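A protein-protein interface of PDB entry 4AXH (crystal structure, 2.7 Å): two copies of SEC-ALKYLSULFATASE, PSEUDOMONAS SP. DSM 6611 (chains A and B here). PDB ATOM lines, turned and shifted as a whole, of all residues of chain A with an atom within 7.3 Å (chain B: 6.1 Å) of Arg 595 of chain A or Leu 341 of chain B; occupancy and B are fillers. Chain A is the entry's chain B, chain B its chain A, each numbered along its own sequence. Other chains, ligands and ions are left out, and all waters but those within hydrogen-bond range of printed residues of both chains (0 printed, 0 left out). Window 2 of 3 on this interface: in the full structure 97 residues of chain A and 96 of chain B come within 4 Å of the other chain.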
ATOM      1  N   ASN A 573     -36.649  -1.699 -26.719  1.00  0.00           N
ATOM      2  CA  ASN A 573     -36.087  -3.054 -26.701  1.00  0.00           C
ATOM      3  C   ASN A 573     -36.262  -3.616 -28.099  1.00  0.00           C
ATOM      4  O   ASN A 573     -37.260  -3.321 -28.758  1.00  0.00           O
ATOM      5  CB  ASN A 573     -36.778  -3.953 -25.675  1.00  0.00           C
ATOM      6  CG  ASN A 573     -36.279  -3.747 -24.273  1.00  0.00           C
ATOM      7  OD1 ASN A 573     -35.173  -3.234 -24.029  1.00  0.00           O
ATOM      8  ND2 ASN A 573     -37.065  -4.189 -23.311  1.00  0.00           N
ATOM      9  N   GLN A 581     -30.714 -12.856 -29.891  1.00  0.00           N
ATOM     10  CA  GLN A 581     -30.041 -11.658 -29.397  1.00  0.00           C
ATOM     11  C   GLN A 581     -31.013 -10.523 -29.056  1.00  0.00           C
ATOM     12  O   GLN A 581     -31.859 -10.135 -29.874  1.00  0.00           O
ATOM     13  CB  GLN A 581     -28.967 -11.186 -30.402  1.00  0.00           C
ATOM     14  CG  GLN A 581     -27.839 -10.391 -29.756  1.00  0.00           C
ATOM     15  CD  GLN A 581     -27.506  -9.153 -30.541  1.00  0.00           C
ATOM     16  OE1 GLN A 581     -26.865  -9.203 -31.597  1.00  0.00           O
ATOM     17  NE2 GLN A 581     -27.933  -8.005 -30.036  1.00  0.00           N
ATOM     18  N   ASP A 582     -30.852  -9.982 -27.849  1.00  0.00           N
ATOM     19  CA  ASP A 582     -31.661  -8.895 -27.324  1.00  0.00           C
ATOM     20  C   ASP A 582     -30.813  -7.635 -27.198  1.00  0.00           C
ATOM     21  O   ASP A 582     -29.707  -7.678 -26.660  1.00  0.00           O
ATOM     22  CB  ASP A 582     -32.254  -9.281 -25.969  1.00  0.00           C
ATOM     23  CG  ASP A 582     -33.255 -10.406 -26.069  1.00  0.00           C
ATOM     24  OD1 ASP A 582     -32.834 -11.581 -26.002  1.00  0.00           O
ATOM     25  OD2 ASP A 582     -34.455 -10.115 -26.230  1.00  0.00           O
ATOM     26  N   ILE A 583     -31.324  -6.520 -27.713  1.00  0.00           N
ATOM     27  CA  ILE A 583     -30.605  -5.262 -27.663  1.00  0.00           C
ATOM     28  C   ILE A 583     -31.503  -4.163 -27.117  1.00  0.00           C
ATOM     29  O   ILE A 583     -32.626  -4.004 -27.577  1.00  0.00           O
ATOM     30  CB  ILE A 583     -29.819  -4.959 -28.996  1.00  0.00           C
ATOM     31  CG1 ILE A 583     -29.066  -3.607 -28.997  1.00  0.00           C
ATOM     32  CG2 ILE A 583     -30.598  -5.228 -30.290  1.00  0.00           C
ATOM     33  CD1 ILE A 583     -29.892  -2.336 -29.221  1.00  0.00           C
ATOM     34  N   ALA A 584     -31.025  -3.432 -26.105  1.00  0.00           N
ATOM     35  CA  ALA A 584     -31.774  -2.365 -25.453  1.00  0.00           C
ATOM     36  C   ALA A 584     -31.294  -0.953 -25.821  1.00  0.00           C
ATOM     37  O   ALA A 584     -30.272  -0.480 -25.298  1.00  0.00           O
ATOM     38  CB  ALA A 584     -31.781  -2.571 -23.948  1.00  0.00           C
ATOM     39  N   LEU A 585     -32.046  -0.272 -26.728  1.00  0.00           N
ATOM     40  CA  LEU A 585     -31.759   1.112 -27.118  1.00  0.00           C
ATOM     41  C   LEU A 585     -32.309   2.051 -26.086  1.00  0.00           C
ATOM     42  O   LEU A 585     -33.257   1.721 -25.375  1.00  0.00           O
ATOM     43  CB  LEU A 585     -32.367   1.510 -28.451  1.00  0.00           C
ATOM     44  CG  LEU A 585     -31.863   0.871 -29.721  1.00  0.00           C
ATOM     45  CD1 LEU A 585     -32.555   1.530 -30.933  1.00  0.00           C
ATOM     46  CD2 LEU A 585     -30.369   1.046 -29.888  1.00  0.00           C
ATOM     47  N   THR A 586     -31.688   3.229 -25.986  1.00  0.00           N
ATOM     48  CA  THR A 586     -32.073   4.332 -25.105  1.00  0.00           C
ATOM     49  C   THR A 586     -31.769   5.639 -25.800  1.00  0.00           C
ATOM     50  O   THR A 586     -30.674   5.800 -26.325  1.00  0.00           O
ATOM     51  CB  THR A 586     -31.588   4.186 -23.631  1.00  0.00           C
ATOM     52  OG1 THR A 586     -31.232   5.470 -23.124  1.00  0.00           O
ATOM     53  CG2 THR A 586     -30.464   3.150 -23.431  1.00  0.00           C
ATOM     54  N   ARG A 588     -31.819   9.588 -25.130  1.00  0.00           N
ATOM     55  CA  ARG A 588     -31.841  10.570 -24.052  1.00  0.00           C
ATOM     56  C   ARG A 588     -31.044  11.783 -24.484  1.00  0.00           C
ATOM     57  O   ARG A 588     -29.913  11.641 -24.965  1.00  0.00           O
ATOM     58  CB  ARG A 588     -31.218   9.957 -22.782  1.00  0.00           C
ATOM     59  CG  ARG A 588     -31.756  10.557 -21.503  1.00  0.00           C
ATOM     60  CD  ARG A 588     -31.293   9.778 -20.279  1.00  0.00           C
ATOM     61  NE  ARG A 588     -29.987  10.269 -19.861  1.00  0.00           N
ATOM     62  CZ  ARG A 588     -29.749  10.969 -18.766  1.00  0.00           C
ATOM     63  NH1 ARG A 588     -30.699  11.151 -17.873  1.00  0.00           N
ATOM     64  NH2 ARG A 588     -28.543  11.437 -18.527  1.00  0.00           N
ATOM     65  N   THR A 593     -27.843   5.583 -27.289  1.00  0.00           N
ATOM     66  CA  THR A 593     -26.890   4.638 -26.696  1.00  0.00           C
ATOM     67  C   THR A 593     -27.546   3.222 -26.746  1.00  0.00           C
ATOM     68  O   THR A 593     -28.773   3.113 -26.903  1.00  0.00           O
ATOM     69  CB  THR A 593     -26.445   5.086 -25.288  1.00  0.00           C
ATOM     70  OG1 THR A 593     -27.580   5.362 -24.451  1.00  0.00           O
ATOM     71  CG2 THR A 593     -25.553   6.315 -25.338  1.00  0.00           C
ATOM     72  N   GLN A 594     -26.737   2.152 -26.659  1.00  0.00           N
ATOM     73  CA  GLN A 594     -27.252   0.789 -26.731  1.00  0.00           C
ATOM     74  C   GLN A 594     -26.516  -0.170 -25.809  1.00  0.00           C
ATOM     75  O   GLN A 594     -25.359   0.070 -25.432  1.00  0.00           O
ATOM     76  CB  GLN A 594     -27.220   0.271 -28.178  1.00  0.00           C
ATOM     77  CG  GLN A 594     -25.817   0.051 -28.795  1.00  0.00           C
ATOM     78  CD  GLN A 594     -25.834  -0.761 -30.076  1.00  0.00           C
ATOM     79  OE1 GLN A 594     -26.728  -1.590 -30.321  1.00  0.00           O
ATOM     80  NE2 GLN A 594     -24.819  -0.570 -30.916  1.00  0.00           N
ATOM     81  N   ARG A 595     -27.201  -1.264 -25.447  1.00  0.00           N
ATOM     82  CA  ARG A 595     -26.688  -2.323 -24.584  1.00  0.00           C
ATOM     83  C   ARG A 595     -27.011  -3.642 -25.261  1.00  0.00           C
ATOM     84  O   ARG A 595     -28.174  -4.032 -25.303  1.00  0.00           O
ATOM     85  CB  ARG A 595     -27.355  -2.295 -23.217  1.00  0.00           C
ATOM     86  CG  ARG A 595     -27.037  -1.108 -22.348  1.00  0.00           C
ATOM     87  CD  ARG A 595     -27.852  -1.167 -21.073  1.00  0.00           C
ATOM     88  NE  ARG A 595     -27.673   0.032 -20.255  1.00  0.00           N
ATOM     89  CZ  ARG A 595     -28.233   0.205 -19.066  1.00  0.00           C
ATOM     90  NH1 ARG A 595     -29.011  -0.740 -18.548  1.00  0.00           N
ATOM     91  NH2 ARG A 595     -28.002   1.311 -18.373  1.00  0.00           N
ATOM     92  N   VAL A 596     -25.980  -4.316 -25.809  1.00  0.00           N
ATOM     93  CA  VAL A 596     -26.100  -5.603 -26.476  1.00  0.00           C
ATOM     94  C   VAL A 596     -26.203  -6.671 -25.383  1.00  0.00           C
ATOM     95  O   VAL A 596     -25.472  -6.594 -24.384  1.00  0.00           O
ATOM     96  CB  VAL A 596     -24.932  -5.846 -27.461  1.00  0.00           C
ATOM     97  CG1 VAL A 596     -25.091  -7.179 -28.189  1.00  0.00           C
ATOM     98  CG2 VAL A 596     -24.819  -4.696 -28.472  1.00  0.00           C
ATOM     99  N   GLY A 597     -27.171  -7.584 -25.545  1.00  0.00           N
ATOM    100  CA  GLY A 597     -27.436  -8.661 -24.595  1.00  0.00           C
ATOM    101  C   GLY A 597     -28.311  -8.275 -23.421  1.00  0.00           C
ATOM    102  O   GLY A 597     -28.533  -9.078 -22.513  1.00  0.00           O
ATOM    103  N   SER A 598     -28.818  -7.044 -23.423  1.00  0.00           N
ATOM    104  CA  SER A 598     -29.658  -6.536 -22.349  1.00  0.00           C
ATOM    105  C   SER A 598     -31.088  -6.300 -22.866  1.00  0.00           C
ATOM    106  O   SER A 598     -31.339  -6.367 -24.071  1.00  0.00           O
ATOM    107  CB  SER A 598     -29.056  -5.243 -21.796  1.00  0.00           C
ATOM    108  OG  SER A 598     -29.685  -4.803 -20.603  1.00  0.00           O
ATOM    109  N   LEU A 599     -32.024  -6.085 -21.925  1.00  0.00           N
ATOM    110  CA  LEU A 599     -33.417  -5.727 -22.147  1.00  0.00           C
ATOM    111  C   LEU A 599     -33.822  -4.796 -21.010  1.00  0.00           C
ATOM    112  O   LEU A 599     -33.674  -5.163 -19.842  1.00  0.00           O
ATOM    113  CB  LEU A 599     -34.353  -6.958 -22.191  1.00  0.00           C
ATOM    114  CG  LEU A 599     -34.371  -7.821 -23.459  1.00  0.00           C
ATOM    115  CD1 LEU A 599     -35.020  -9.151 -23.173  1.00  0.00           C
ATOM    116  CD2 LEU A 599     -35.086  -7.139 -24.614  1.00  0.00           C
ATOM    117  N   ASN A 600     -34.297  -3.579 -21.344  1.00  0.00           N
ATOM    118  CA  ASN A 600     -34.749  -2.650 -20.313  1.00  0.00           C
ATOM    119  C   ASN A 600     -36.083  -3.151 -19.758  1.00  0.00           C
ATOM    120  O   ASN A 600     -36.989  -3.476 -20.535  1.00  0.00           O
ATOM    121  CB  ASN A 600     -34.887  -1.234 -20.831  1.00  0.00           C
ATOM    122  CG  ASN A 600     -34.899  -0.218 -19.707  1.00  0.00           C
ATOM    123  OD1 ASN A 600     -35.932   0.027 -19.052  1.00  0.00           O
ATOM    124  ND2 ASN A 600     -33.725   0.347 -19.418  1.00  0.00           N
ATOM    125  N   PRO A 601     -36.219  -3.296 -18.435  1.00  0.00           N
ATOM    126  CA  PRO A 601     -37.487  -3.825 -17.896  1.00  0.00           C
ATOM    127  C   PRO A 601     -38.672  -2.867 -18.051  1.00  0.00           C
ATOM    128  O   PRO A 601     -39.813  -3.321 -18.158  1.00  0.00           O
ATOM    129  CB  PRO A 601     -37.160  -4.133 -16.423  1.00  0.00           C
ATOM    130  CG  PRO A 601     -35.656  -3.947 -16.281  1.00  0.00           C
ATOM    131  CD  PRO A 601     -35.257  -2.997 -17.357  1.00  0.00           C
ATOM    132  N   LEU B 306     -19.442   3.152  -5.560  1.00  0.00           N
ATOM    133  CA  LEU B 306     -18.760   2.918  -6.832  1.00  0.00           C
ATOM    134  C   LEU B 306     -17.667   3.950  -7.044  1.00  0.00           C
ATOM    135  O   LEU B 306     -17.898   5.151  -6.865  1.00  0.00           O
ATOM    136  CB  LEU B 306     -19.739   2.854  -8.021  1.00  0.00           C
ATOM    137  CG  LEU B 306     -19.148   2.745  -9.438  1.00  0.00           C
ATOM    138  CD1 LEU B 306     -18.566   1.376  -9.697  1.00  0.00           C
ATOM    139  CD2 LEU B 306     -20.156   3.077 -10.470  1.00  0.00           C
ATOM    140  N   TYR B 336     -18.183   2.239 -21.490  1.00  0.00           N
ATOM    141  CA  TYR B 336     -17.704   1.817 -20.170  1.00  0.00           C
ATOM    142  C   TYR B 336     -18.487   2.492 -19.030  1.00  0.00           C
ATOM    143  O   TYR B 336     -18.647   1.923 -17.945  1.00  0.00           O
ATOM    144  CB  TYR B 336     -16.201   2.114 -20.036  1.00  0.00           C
ATOM    145  CG  TYR B 336     -15.295   1.204 -20.845  1.00  0.00           C
ATOM    146  CD1 TYR B 336     -15.439  -0.179 -20.792  1.00  0.00           C
ATOM    147  CD2 TYR B 336     -14.251   1.720 -21.601  1.00  0.00           C
ATOM    148  CE1 TYR B 336     -14.600  -1.023 -21.503  1.00  0.00           C
ATOM    149  CE2 TYR B 336     -13.409   0.885 -22.327  1.00  0.00           C
ATOM    150  CZ  TYR B 336     -13.585  -0.489 -22.269  1.00  0.00           C
ATOM    151  OH  TYR B 336     -12.729  -1.339 -22.918  1.00  0.00           O
ATOM    152  N   ILE B 337     -18.935   3.730 -19.260  1.00  0.00           N
ATOM    153  CA  ILE B 337     -19.741   4.475 -18.289  1.00  0.00           C
ATOM    154  C   ILE B 337     -21.088   3.727 -18.173  1.00  0.00           C
ATOM    155  O   ILE B 337     -21.506   3.381 -17.070  1.00  0.00           O
ATOM    156  CB  ILE B 337     -19.908   5.985 -18.696  1.00  0.00           C
ATOM    157  CG1 ILE B 337     -18.565   6.736 -18.569  1.00  0.00           C
ATOM    158  CG2 ILE B 337     -20.984   6.643 -17.827  1.00  0.00           C
ATOM    159  CD1 ILE B 337     -18.437   8.049 -19.245  1.00  0.00           C
ATOM    160  N   ASP B 338     -21.698   3.400 -19.340  1.00  0.00           N
ATOM    161  CA  ASP B 338     -22.969   2.689 -19.460  1.00  0.00           C
ATOM    162  C   ASP B 338     -22.889   1.297 -18.865  1.00  0.00           C
ATOM    163  O   ASP B 338     -23.829   0.878 -18.194  1.00  0.00           O
ATOM    164  CB  ASP B 338     -23.379   2.647 -20.932  1.00  0.00           C
ATOM    165  CG  ASP B 338     -24.801   2.218 -21.226  1.00  0.00           C
ATOM    166  OD1 ASP B 338     -25.717   2.623 -20.457  1.00  0.00           O
ATOM    167  OD2 ASP B 338     -25.012   1.567 -22.291  1.00  0.00           O
ATOM    168  N   ALA B 339     -21.758   0.585 -19.064  1.00  0.00           N
ATOM    169  CA  ALA B 339     -21.572  -0.754 -18.488  1.00  0.00           C
ATOM    170  C   ALA B 339     -21.463  -0.654 -16.977  1.00  0.00           C
ATOM    171  O   ALA B 339     -21.987  -1.528 -16.261  1.00  0.00           O
ATOM    172  CB  ALA B 339     -20.365  -1.433 -19.080  1.00  0.00           C
ATOM    173  N   SER B 340     -20.881   0.447 -16.481  1.00  0.00           N
ATOM    174  CA  SER B 340     -20.840   0.676 -15.045  1.00  0.00           C
ATOM    175  C   SER B 340     -22.259   1.034 -14.526  1.00  0.00           C
ATOM    176  O   SER B 340     -22.620   0.597 -13.444  1.00  0.00           O
ATOM    177  CB  SER B 340     -19.787   1.726 -14.671  1.00  0.00           C
ATOM    178  OG  SER B 340     -20.243   3.070 -14.688  1.00  0.00           O
ATOM    179  N   LEU B 341     -23.078   1.755 -15.324  1.00  0.00           N
ATOM    180  CA  LEU B 341     -24.448   2.109 -14.930  1.00  0.00           C
ATOM    181  C   LEU B 341     -25.321   0.864 -14.764  1.00  0.00           C
ATOM    182  O   LEU B 341     -26.024   0.740 -13.760  1.00  0.00           O
ATOM    183  CB  LEU B 341     -25.110   3.109 -15.917  1.00  0.00           C
ATOM    184  CG  LEU B 341     -26.568   3.636 -15.586  1.00  0.00           C
ATOM    185  CD1 LEU B 341     -26.666   4.230 -14.183  1.00  0.00           C
ATOM    186  CD2 LEU B 341     -26.970   4.728 -16.560  1.00  0.00           C
ATOM    187  N   GLU B 342     -25.277  -0.042 -15.761  1.00  0.00           N
ATOM    188  CA  GLU B 342     -26.037  -1.272 -15.765  1.00  0.00           C
ATOM    189  C   GLU B 342     -25.588  -2.219 -14.652  1.00  0.00           C
ATOM    190  O   GLU B 342     -26.436  -2.686 -13.914  1.00  0.00           O
ATOM    191  CB  GLU B 342     -25.927  -1.906 -17.147  1.00  0.00           C
ATOM    192  CG  GLU B 342     -26.539  -3.296 -17.275  1.00  0.00           C
ATOM    193  CD  GLU B 342     -26.557  -3.849 -18.690  1.00  0.00           C
ATOM    194  OE1 GLU B 342     -25.738  -3.405 -19.533  1.00  0.00           O
ATOM    195  OE2 GLU B 342     -27.421  -4.717 -18.960  1.00  0.00           O
ATOM    196  N   LYS B 343     -24.265  -2.454 -14.487  1.00  0.00           N
ATOM    197  CA  LYS B 343     -23.750  -3.373 -13.466  1.00  0.00           C
ATOM    198  C   LYS B 343     -23.840  -2.891 -12.022  1.00  0.00           C
ATOM    199  O   LYS B 343     -24.003  -3.712 -11.108  1.00  0.00           O
ATOM    200  CB  LYS B 343     -22.314  -3.820 -13.791  1.00  0.00           C
ATOM    201  CG  LYS B 343     -22.201  -5.188 -14.479  1.00  0.00           C
ATOM    202  CD  LYS B 343     -21.507  -6.212 -13.564  1.00  0.00           C
ATOM    203  CE  LYS B 343     -21.111  -7.513 -14.238  1.00  0.00           C
ATOM    204  NZ  LYS B 343     -22.265  -8.443 -14.395  1.00  0.00           N
ATOM    205  N   TYR B 344     -23.699  -1.576 -11.794  1.00  0.00           N
ATOM    206  CA  TYR B 344     -23.644  -1.047 -10.428  1.00  0.00           C
ATOM    207  C   TYR B 344     -24.665  -0.004 -10.041  1.00  0.00           C
ATOM    208  O   TYR B 344     -24.871   0.179  -8.843  1.00  0.00           O
ATOM    209  CB  TYR B 344     -22.214  -0.567 -10.076  1.00  0.00           C
ATOM    210  CG  TYR B 344     -21.130  -1.541 -10.478  1.00  0.00           C
ATOM    211  CD1 TYR B 344     -21.035  -2.795  -9.876  1.00  0.00           C
ATOM    212  CD2 TYR B 344     -20.246  -1.242 -11.511  1.00  0.00           C
ATOM    213  CE1 TYR B 344     -20.057  -3.709 -10.264  1.00  0.00           C
ATOM    214  CE2 TYR B 344     -19.266  -2.151 -11.912  1.00  0.00           C
ATOM    215  CZ  TYR B 344     -19.174  -3.383 -11.283  1.00  0.00           C
ATOM    216  OH  TYR B 344     -18.234  -4.298 -11.689  1.00  0.00           O
ATOM    217  N   GLY B 345     -25.292   0.643 -11.017  1.00  0.00           N
ATOM    218  CA  GLY B 345     -26.279   1.697 -10.812  1.00  0.00           C
ATOM    219  C   GLY B 345     -27.368   1.428  -9.796  1.00  0.00           C
ATOM    220  O   GLY B 345     -27.658   2.287  -8.964  1.00  0.00           O
ATOM    221  N   ASP B 346     -27.945   0.211  -9.828  1.00  0.00           N
ATOM    222  CA  ASP B 346     -29.007  -0.205  -8.893  1.00  0.00           C
ATOM    223  C   ASP B 346     -28.481  -0.630  -7.514  1.00  0.00           C
ATOM    224  O   ASP B 346     -29.267  -0.644  -6.554  1.00  0.00           O
ATOM    225  CB  ASP B 346     -29.861  -1.323  -9.498  1.00  0.00           C
ATOM    226  CG  ASP B 346     -30.346  -1.061 -10.919  1.00  0.00           C
ATOM    227  OD1 ASP B 346     -30.709   0.107 -11.221  1.00  0.00           O
ATOM    228  OD2 ASP B 346     -30.365  -2.022 -11.726  1.00  0.00           O
ATOM    229  N   VAL B 365     -26.764   9.426  -8.518  1.00  0.00           N
ATOM    230  CA  VAL B 365     -25.667   8.686  -9.145  1.00  0.00           C
ATOM    231  C   VAL B 365     -26.075   8.163 -10.519  1.00  0.00           C
ATOM    232  O   VAL B 365     -25.293   8.267 -11.462  1.00  0.00           O
ATOM    233  CB  VAL B 365     -24.854   7.657  -8.277  1.00  0.00           C
ATOM    234  CG1 VAL B 365     -24.763   8.048  -6.806  1.00  0.00           C
ATOM    235  CG2 VAL B 365     -25.354   6.234  -8.424  1.00  0.00           C
ATOM    236  N   ARG B 366     -27.291   7.616 -10.640  1.00  0.00           N
ATOM    237  CA  ARG B 366     -27.835   7.070 -11.902  1.00  0.00           C
ATOM    238  C   ARG B 366     -28.008   8.145 -12.982  1.00  0.00           C
ATOM    239  O   ARG B 366     -27.700   7.889 -14.152  1.00  0.00           O
ATOM    240  CB  ARG B 366     -29.161   6.364 -11.659  1.00  0.00           C
ATOM    241  CG  ARG B 366     -29.011   4.959 -11.162  1.00  0.00           C
ATOM    242  CD  ARG B 366     -30.343   4.458 -10.638  1.00  0.00           C
ATOM    243  NE  ARG B 366     -30.118   3.731  -9.397  1.00  0.00           N
ATOM    244  CZ  ARG B 366     -30.758   3.953  -8.262  1.00  0.00           C
ATOM    245  NH1 ARG B 366     -31.732   4.856  -8.207  1.00  0.00           N
ATOM    246  NH2 ARG B 366     -30.456   3.251  -7.177  1.00  0.00           N
ATOM    247  N   THR B 367     -28.496   9.352 -12.582  1.00  0.00           N
ATOM    248  CA  THR B 367     -28.648  10.495 -13.471  1.00  0.00           C
ATOM    249  C   THR B 367     -27.238  10.958 -13.902  1.00  0.00           C
ATOM    250  O   THR B 367     -27.033  11.244 -15.073  1.00  0.00           O
ATOM    251  CB  THR B 367     -29.409  11.629 -12.745  1.00  0.00           C
ATOM    252  OG1 THR B 367     -30.739  11.203 -12.483  1.00  0.00           O
ATOM    253  CG2 THR B 367     -29.402  12.982 -13.512  1.00  0.00           C
ATOM    254  N   LEU B 369     -24.275   9.258 -14.010  1.00  0.00           N
ATOM    255  CA  LEU B 369     -23.740   8.270 -14.947  1.00  0.00           C
ATOM    256  C   LEU B 369     -24.336   8.343 -16.327  1.00  0.00           C
ATOM    257  O   LEU B 369     -23.597   8.396 -17.306  1.00  0.00           O
ATOM    258  CB  LEU B 369     -23.847   6.850 -14.394  1.00  0.00           C
ATOM    259  CG  LEU B 369     -22.873   6.535 -13.270  1.00  0.00           C
ATOM    260  CD1 LEU B 369     -23.021   5.104 -12.828  1.00  0.00           C
ATOM    261  CD2 LEU B 369     -21.442   6.880 -13.686  1.00  0.00           C
ATOM    262  N   ALA B 370     -25.660   8.405 -16.428  1.00  0.00           N
ATOM    263  CA  ALA B 370     -26.331   8.488 -17.706  1.00  0.00           C
ATOM    264  C   ALA B 370     -25.991   9.772 -18.432  1.00  0.00           C
ATOM    265  O   ALA B 370     -25.816   9.736 -19.644  1.00  0.00           O
ATOM    266  CB  ALA B 370     -27.814   8.363 -17.508  1.00  0.00           C
ATOM    267  N   ARG B 373     -22.260   9.298 -19.704  1.00  0.00           N
ATOM    268  CA  ARG B 373     -22.370   8.397 -20.852  1.00  0.00           C
ATOM    269  C   ARG B 373     -22.854   9.169 -22.064  1.00  0.00           C
ATOM    270  O   ARG B 373     -22.144   9.227 -23.048  1.00  0.00           O
ATOM    271  CB  ARG B 373     -23.346   7.232 -20.545  1.00  0.00           C
ATOM    272  CG  ARG B 373     -23.740   6.443 -21.795  1.00  0.00           C
ATOM    273  CD  ARG B 373     -25.081   5.773 -21.667  1.00  0.00           C
ATOM    274  NE  ARG B 373     -26.193   6.716 -21.708  1.00  0.00           N
ATOM    275  CZ  ARG B 373     -27.359   6.515 -21.108  1.00  0.00           C
ATOM    276  NH1 ARG B 373     -27.578   5.404 -20.432  1.00  0.00           N
ATOM    277  NH2 ARG B 373     -28.314   7.430 -21.176  1.00  0.00           N
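No position is printed for both chains.
Among the printed residues, merely in contact across the chains: Arg 588 of chain A with Thr 367 of chain B (3.8 Å), Arg 588 of chain A with Arg 373 of chain B (3.5 Å), Arg 595 of chain A with Leu 341 of chain B (3.9 Å) and Arg 595 of chain A with Glu 342 of chain B (3.4 Å).
Of the printed residues of chain B, Arg 588 of chain A touches Thr 367 (3.8 Å), Ala 370 (3.0 Å) and Arg 373 (3.5 Å). Printed residues of chain B within 4 Å of Ser 598 of chain A: Glu 342. Of chain A, only Arg 595 (3.9 Å) comes within 4 Å of Leu 341 of chain B. Printed residues of chain A within 4 Å of Glu 342 of chain B: Arg 595 and Ser 598. Of the printed residues of chain A, Arg 373 of chain B touches Arg 588 (3.5 Å) and Thr 593 (3.4 Å). The nearest residue of chain B that does not touch Arg 595 of chain A is Arg 373 of chain B (4.6 Å).
Printed residues of chain A that touch a printed residue of chain B: Arg 588, Thr 593, Gln 594, Arg 595 and Ser 598. Of the 18 printed residues of chain B, 6 touch a printed residue of chain A. Hydrophobic or aromatic side chains of chain B that line the printed part of chain A: Leu 341 and Ala 370. Among the printed residues, 9 pairs touch across the chains.
The guanidinium group of Arg 595 of chain A lies within salt-bridge range of the side-chain carboxylate of Asp 338 of chain B (3.3 Å). OG of Ser 598 of chain A sits at hydrogen-bond distance from OE2 of Glu 342 of chain B. The backbone carbonyl oxygen (O) of Ala 370 of chain B lies close to the guanidinium group (NH2) of Arg 588 of chain A, at 3.4 Å. The guanidinium group (NE) of Arg 373 of chain B is in hydrogen-bond range of the side-chain hydroxyl (OG1) of Thr 593 of chain A (3.4 Å). The backbone carbonyl oxygen of Gln 594 of chain A sits close to the side-chain carboxylate of Asp 338 of chain B (3.5 Å).
The side-chain carboxylate (OD1) of Asp 338 of chain B is in salt-bridge range of the guanidinium group (NH1) of Arg 373 of chain B (3.3 Å). The backbone NH (N) of Ser 598 of chain A is in hydrogen-bond range of the backbone carbonyl oxygen (O) of Asp 582 of chain A. O of Arg 595 of chain A lies within hydrogen-bond range of N of Ala 584 of chain A (3.0 Å). O of Thr 586 of chain A is in hydrogen-bond range of N of Thr 593 of chain A (3.0 Å).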
